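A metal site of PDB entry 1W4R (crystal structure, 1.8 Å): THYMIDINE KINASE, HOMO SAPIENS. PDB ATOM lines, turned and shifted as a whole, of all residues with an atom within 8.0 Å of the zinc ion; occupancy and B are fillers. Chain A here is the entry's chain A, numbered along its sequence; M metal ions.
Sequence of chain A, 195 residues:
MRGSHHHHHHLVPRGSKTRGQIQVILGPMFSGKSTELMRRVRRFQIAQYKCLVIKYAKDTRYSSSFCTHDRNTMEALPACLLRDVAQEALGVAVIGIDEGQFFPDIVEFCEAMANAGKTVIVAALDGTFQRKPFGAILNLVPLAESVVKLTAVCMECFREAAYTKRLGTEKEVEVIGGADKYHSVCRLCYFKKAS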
ATOM      1  N   VAL A 153      10.052   0.526   9.675  1.00  0.00           N
ATOM      2  CA  VAL A 153      11.228  -0.205   9.212  1.00  0.00           C
ATOM      3  C   VAL A 153      10.699  -1.365   8.386  1.00  0.00           C
ATOM      4  O   VAL A 153       9.749  -2.029   8.794  1.00  0.00           O
ATOM      5  CB  VAL A 153      12.071  -0.714  10.381  1.00  0.00           C
ATOM      6  CG1 VAL A 153      13.183  -1.630   9.898  1.00  0.00           C
ATOM      7  CG2 VAL A 153      12.629   0.460  11.153  1.00  0.00           C
ATOM      8  N   CYS A 154      11.275  -1.573   7.209  1.00  0.00           N
ATOM      9  CA  CYS A 154      10.839  -2.638   6.338  1.00  0.00           C
ATOM     10  C   CYS A 154      11.176  -3.931   7.054  1.00  0.00           C
ATOM     11  O   CYS A 154      12.335  -4.116   7.442  1.00  0.00           O
ATOM     12  CB  CYS A 154      11.573  -2.589   5.000  1.00  0.00           C
ATOM     13  SG  CYS A 154      11.071  -3.939   3.920  1.00  0.00           S
ATOM     14  N   MET A 155      10.189  -4.809   7.201  1.00  0.00           N
ATOM     15  CA  MET A 155      10.398  -6.012   7.974  1.00  0.00           C
ATOM     16  C   MET A 155      11.086  -7.094   7.138  1.00  0.00           C
ATOM     17  O   MET A 155      11.384  -8.162   7.667  1.00  0.00           O
ATOM     18  CB  MET A 155       9.075  -6.515   8.535  1.00  0.00           C
ATOM     19  CG  MET A 155       8.556  -5.669   9.669  1.00  0.00           C
ATOM     20  SD  MET A 155       6.882  -6.096  10.117  1.00  0.00           S
ATOM     21  CE  MET A 155       6.680  -5.072  11.563  1.00  0.00           C
ATOM     22  N   GLU A 156      11.358  -6.808   5.875  1.00  0.00           N
ATOM     23  CA  GLU A 156      11.936  -7.793   4.955  1.00  0.00           C
ATOM     24  C   GLU A 156      13.356  -7.429   4.578  1.00  0.00           C
ATOM     25  O   GLU A 156      14.174  -8.323   4.395  1.00  0.00           O
ATOM     26  CB  GLU A 156      10.999  -8.036   3.765  1.00  0.00           C
ATOM     27  CG  GLU A 156       9.640  -8.533   4.274  1.00  0.00           C
ATOM     28  CD  GLU A 156       8.579  -8.842   3.235  1.00  0.00           C
ATOM     29  OE1 GLU A 156       8.860  -8.789   2.036  1.00  0.00           O
ATOM     30  OE2 GLU A 156       7.410  -9.165   3.633  1.00  0.00           O
ATOM     31  N   CYS A 157      13.693  -6.141   4.505  1.00  0.00           N
ATOM     32  CA  CYS A 157      15.051  -5.708   4.132  1.00  0.00           C
ATOM     33  C   CYS A 157      15.650  -4.624   5.050  1.00  0.00           C
ATOM     34  O   CYS A 157      16.813  -4.244   4.922  1.00  0.00           O
ATOM     35  CB  CYS A 157      15.064  -5.215   2.680  1.00  0.00           C
ATOM     36  SG  CYS A 157      14.598  -3.472   2.469  1.00  0.00           S
ATOM     37  N   PHE A 158      14.846  -4.110   5.975  1.00  0.00           N
ATOM     38  CA  PHE A 158      15.299  -3.207   7.028  1.00  0.00           C
ATOM     39  C   PHE A 158      15.656  -1.771   6.597  1.00  0.00           C
ATOM     40  O   PHE A 158      16.139  -0.980   7.407  1.00  0.00           O
ATOM     41  CB  PHE A 158      16.371  -3.916   7.909  1.00  0.00           C
ATOM     42  CG  PHE A 158      15.966  -5.304   8.274  1.00  0.00           C
ATOM     43  CD1 PHE A 158      14.866  -5.505   9.109  1.00  0.00           C
ATOM     44  CD2 PHE A 158      16.568  -6.402   7.683  1.00  0.00           C
ATOM     45  CE1 PHE A 158      14.422  -6.787   9.421  1.00  0.00           C
ATOM     46  CE2 PHE A 158      16.130  -7.699   7.977  1.00  0.00           C
ATOM     47  CZ  PHE A 158      15.046  -7.885   8.858  1.00  0.00           C
ATOM     48  N   ARG A 159      15.380  -1.426   5.341  1.00  0.00           N
ATOM     49  CA  ARG A 159      15.399  -0.033   4.937  1.00  0.00           C
ATOM     50  C   ARG A 159      14.095   0.631   5.415  1.00  0.00           C
ATOM     51  O   ARG A 159      13.277  -0.009   6.049  1.00  0.00           O
ATOM     52  CB  ARG A 159      15.501   0.073   3.436  1.00  0.00           C
ATOM     53  CG  ARG A 159      16.855  -0.343   2.891  1.00  0.00           C
ATOM     54  CD  ARG A 159      16.940  -0.167   1.396  1.00  0.00           C
ATOM     55  NE  ARG A 159      17.805  -1.188   0.809  1.00  0.00           N
ATOM     56  CZ  ARG A 159      19.129  -1.207   0.892  1.00  0.00           C
ATOM     57  NH1 ARG A 159      19.798  -0.236   1.528  1.00  0.00           N
ATOM     58  NH2 ARG A 159      19.804  -2.197   0.323  1.00  0.00           N
ATOM     59  N   GLU A 160      13.911   1.907   5.107  1.00  0.00           N
ATOM     60  CA  GLU A 160      12.662   2.614   5.497  1.00  0.00           C
ATOM     61  C   GLU A 160      11.472   2.048   4.722  1.00  0.00           C
ATOM     62  O   GLU A 160      11.548   1.850   3.514  1.00  0.00           O
ATOM     63  CB  GLU A 160      12.759   4.109   5.220  1.00  0.00           C
ATOM     64  CG  GLU A 160      12.901   4.942   6.463  1.00  0.00           C
ATOM     65  CD  GLU A 160      12.771   6.438   6.182  1.00  0.00           C
ATOM     66  OE1 GLU A 160      13.067   6.860   5.052  1.00  0.00           O
ATOM     67  OE2 GLU A 160      12.368   7.194   7.100  1.00  0.00           O
ATOM     68  N   ALA A 161      10.332   1.910   5.410  1.00  0.00           N
ATOM     69  CA  ALA A 161       9.135   1.380   4.831  1.00  0.00           C
ATOM     70  C   ALA A 161       7.999   2.408   4.880  1.00  0.00           C
ATOM     71  O   ALA A 161       7.711   3.011   5.924  1.00  0.00           O
ATOM     72  CB  ALA A 161       8.716   0.120   5.588  1.00  0.00           C
ATOM     73  N   LYS A 165       2.223  -4.510   3.543  1.00  0.00           N
ATOM     74  CA  LYS A 165       1.913  -5.721   2.780  1.00  0.00           C
ATOM     75  C   LYS A 165       1.119  -6.714   3.617  1.00  0.00           C
ATOM     76  O   LYS A 165       1.460  -6.965   4.767  1.00  0.00           O
ATOM     77  CB  LYS A 165       3.249  -6.370   2.343  1.00  0.00           C
ATOM     78  CG  LYS A 165       3.092  -7.719   1.624  1.00  0.00           C
ATOM     79  CD  LYS A 165       4.232  -7.964   0.611  1.00  0.00           C
ATOM     80  CE  LYS A 165       5.457  -8.500   1.256  1.00  0.00           C
ATOM     81  NZ  LYS A 165       6.596  -8.731   0.295  1.00  0.00           N
ATOM     82  N   SER A 184       5.269  -4.143   7.450  1.00  0.00           N
ATOM     83  CA  SER A 184       5.695  -2.854   6.872  1.00  0.00           C
ATOM     84  C   SER A 184       6.800  -3.156   5.880  1.00  0.00           C
ATOM     85  O   SER A 184       7.673  -3.963   6.161  1.00  0.00           O
ATOM     86  CB  SER A 184       6.215  -1.907   7.944  1.00  0.00           C
ATOM     87  OG  SER A 184       6.985  -2.552   8.946  1.00  0.00           O
ATOM     88  N   VAL A 185       6.730  -2.566   4.706  1.00  0.00           N
ATOM     89  CA  VAL A 185       7.676  -2.794   3.626  1.00  0.00           C
ATOM     90  C   VAL A 185       7.973  -1.537   2.833  1.00  0.00           C
ATOM     91  O   VAL A 185       7.148  -0.629   2.733  1.00  0.00           O
ATOM     92  CB  VAL A 185       7.168  -3.854   2.620  1.00  0.00           C
ATOM     93  CG1 VAL A 185       7.091  -5.227   3.299  1.00  0.00           C
ATOM     94  CG2 VAL A 185       5.785  -3.484   2.053  1.00  0.00           C
ATOM     95  N   CYS A 186       9.172  -1.538   2.255  1.00  0.00           N
ATOM     96  CA  CYS A 186       9.590  -0.583   1.246  1.00  0.00           C
ATOM     97  C   CYS A 186       8.982  -0.988  -0.099  1.00  0.00           C
ATOM     98  O   CYS A 186       8.331  -2.008  -0.210  1.00  0.00           O
ATOM     99  CB  CYS A 186      11.101  -0.548   1.217  1.00  0.00           C
ATOM    100  SG  CYS A 186      11.809  -2.068   0.499  1.00  0.00           S
ATOM    101  N   ARG A 187       9.133  -0.124  -1.093  1.00  0.00           N
ATOM    102  CA  ARG A 187       8.577  -0.330  -2.432  1.00  0.00           C
ATOM    103  C   ARG A 187       9.094  -1.663  -3.038  1.00  0.00           C
ATOM    104  O   ARG A 187       8.317  -2.390  -3.652  1.00  0.00           O
ATOM    105  CB  ARG A 187       9.038   0.803  -3.323  1.00  0.00           C
ATOM    106  CG  ARG A 187       8.613   0.706  -4.791  1.00  0.00           C
ATOM    107  CD  ARG A 187       9.045   1.917  -5.566  1.00  0.00           C
ATOM    108  NE  ARG A 187       8.409   3.120  -5.047  1.00  0.00           N
ATOM    109  CZ  ARG A 187       7.219   3.552  -5.422  1.00  0.00           C
ATOM    110  NH1 ARG A 187       6.538   2.954  -6.373  1.00  0.00           N
ATOM    111  NH2 ARG A 187       6.688   4.651  -4.874  1.00  0.00           N
ATOM    112  N   LEU A 188      10.381  -1.916  -2.884  1.00  0.00           N
ATOM    113  CA  LEU A 188      10.994  -3.113  -3.503  1.00  0.00           C
ATOM    114  C   LEU A 188      10.419  -4.370  -2.895  1.00  0.00           C
ATOM    115  O   LEU A 188       9.974  -5.259  -3.622  1.00  0.00           O
ATOM    116  CB  LEU A 188      12.510  -3.071  -3.374  1.00  0.00           C
ATOM    117  CG  LEU A 188      13.303  -2.603  -4.620  1.00  0.00           C
ATOM    118  CD1 LEU A 188      12.492  -1.852  -5.665  1.00  0.00           C
ATOM    119  CD2 LEU A 188      14.566  -1.830  -4.239  1.00  0.00           C
ATOM    120  N   CYS A 189      10.336  -4.419  -1.565  1.00  0.00           N
ATOM    121  CA  CYS A 189       9.766  -5.598  -0.903  1.00  0.00           C
ATOM    122  C   CYS A 189       8.276  -5.731  -1.087  1.00  0.00           C
ATOM    123  O   CYS A 189       7.723  -6.840  -1.097  1.00  0.00           O
ATOM    124  CB  CYS A 189      10.146  -5.607   0.550  1.00  0.00           C
ATOM    125  SG  CYS A 189      11.950  -5.714   0.866  1.00  0.00           S
ATOM    126  N   TYR A 190       7.575  -4.609  -1.275  1.00  0.00           N
ATOM    127  CA  TYR A 190       6.153  -4.677  -1.522  1.00  0.00           C
ATOM    128  C   TYR A 190       5.857  -5.521  -2.768  1.00  0.00           C
ATOM    129  O   TYR A 190       4.902  -6.300  -2.789  1.00  0.00           O
ATOM    130  CB  TYR A 190       5.560  -3.269  -1.699  1.00  0.00           C
ATOM    131  CG  TYR A 190       4.086  -3.304  -1.898  1.00  0.00           C
ATOM    132  CD1 TYR A 190       3.231  -3.392  -0.824  1.00  0.00           C
ATOM    133  CD2 TYR A 190       3.535  -3.319  -3.193  1.00  0.00           C
ATOM    134  CE1 TYR A 190       1.876  -3.480  -1.021  1.00  0.00           C
ATOM    135  CE2 TYR A 190       2.207  -3.392  -3.382  1.00  0.00           C
ATOM    136  CZ  TYR A 190       1.369  -3.473  -2.293  1.00  0.00           C
ATOM    137  OH  TYR A 190       0.023  -3.525  -2.497  1.00  0.00           O
ATOM    138  N   LYS A 192       7.852  -7.692  -4.261  1.00  0.00           N
ATOM    139  CA  LYS A 192       8.330  -9.074  -3.993  1.00  0.00           C
ATOM    140  C   LYS A 192       9.825  -9.104  -4.142  1.00  0.00           C
ATOM    141  O   LYS A 192      10.531  -9.100  -3.124  1.00  0.00           O
ATOM    142  CB  LYS A 192       7.593 -10.196  -4.765  1.00  0.00           C
ATOM    143  CG  LYS A 192       8.426 -10.900  -5.848  1.00  0.00           C
ATOM    144  CD  LYS A 192       7.595 -11.911  -6.657  1.00  0.00           C
ATOM    145  CE  LYS A 192       7.059 -13.053  -5.787  1.00  0.00           C
ATOM    146  NZ  LYS A 192       8.112 -13.551  -4.859  1.00  0.00           N
HETATM  147 ZN    ZN M   1      12.400  -3.735   1.996  1.00  0.00          ZN
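The zinc ion is bound by the side-chain sulfur (SG) of Cys 157 (2.3 Å), the side-chain sulfur (SG) of Cys 186 (2.3 Å), the side-chain sulfur (SG) of Cys 189 (2.3 Å) and the side-chain sulfur (SG) of Cys 154 (2.3 Å).
The zinc ion has four donor atoms within binding distance.
SG of Cys 157 sits close to N of Arg 159 (3.6 Å).
The side-chain sulfur of Cys 186 sits close to the backbone NH of Leu 188, 3.7 Å away.
NZ of Lys 165 lies within hydrogen-bond range of O of Cys 189.
SG of Cys 154 lies close to N of Glu 156, 3.5 Å away.
O of Arg 159 lies within hydrogen-bond range of N of Cys 154 (2.8 Å).
Four residues have an atom within 4 Å of the zinc ion: Cys 154, Cys 157, Cys 186 and Cys 189.
The nearest printed residue that does not touch the zinc ion is Glu 156 (4.6 Å).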
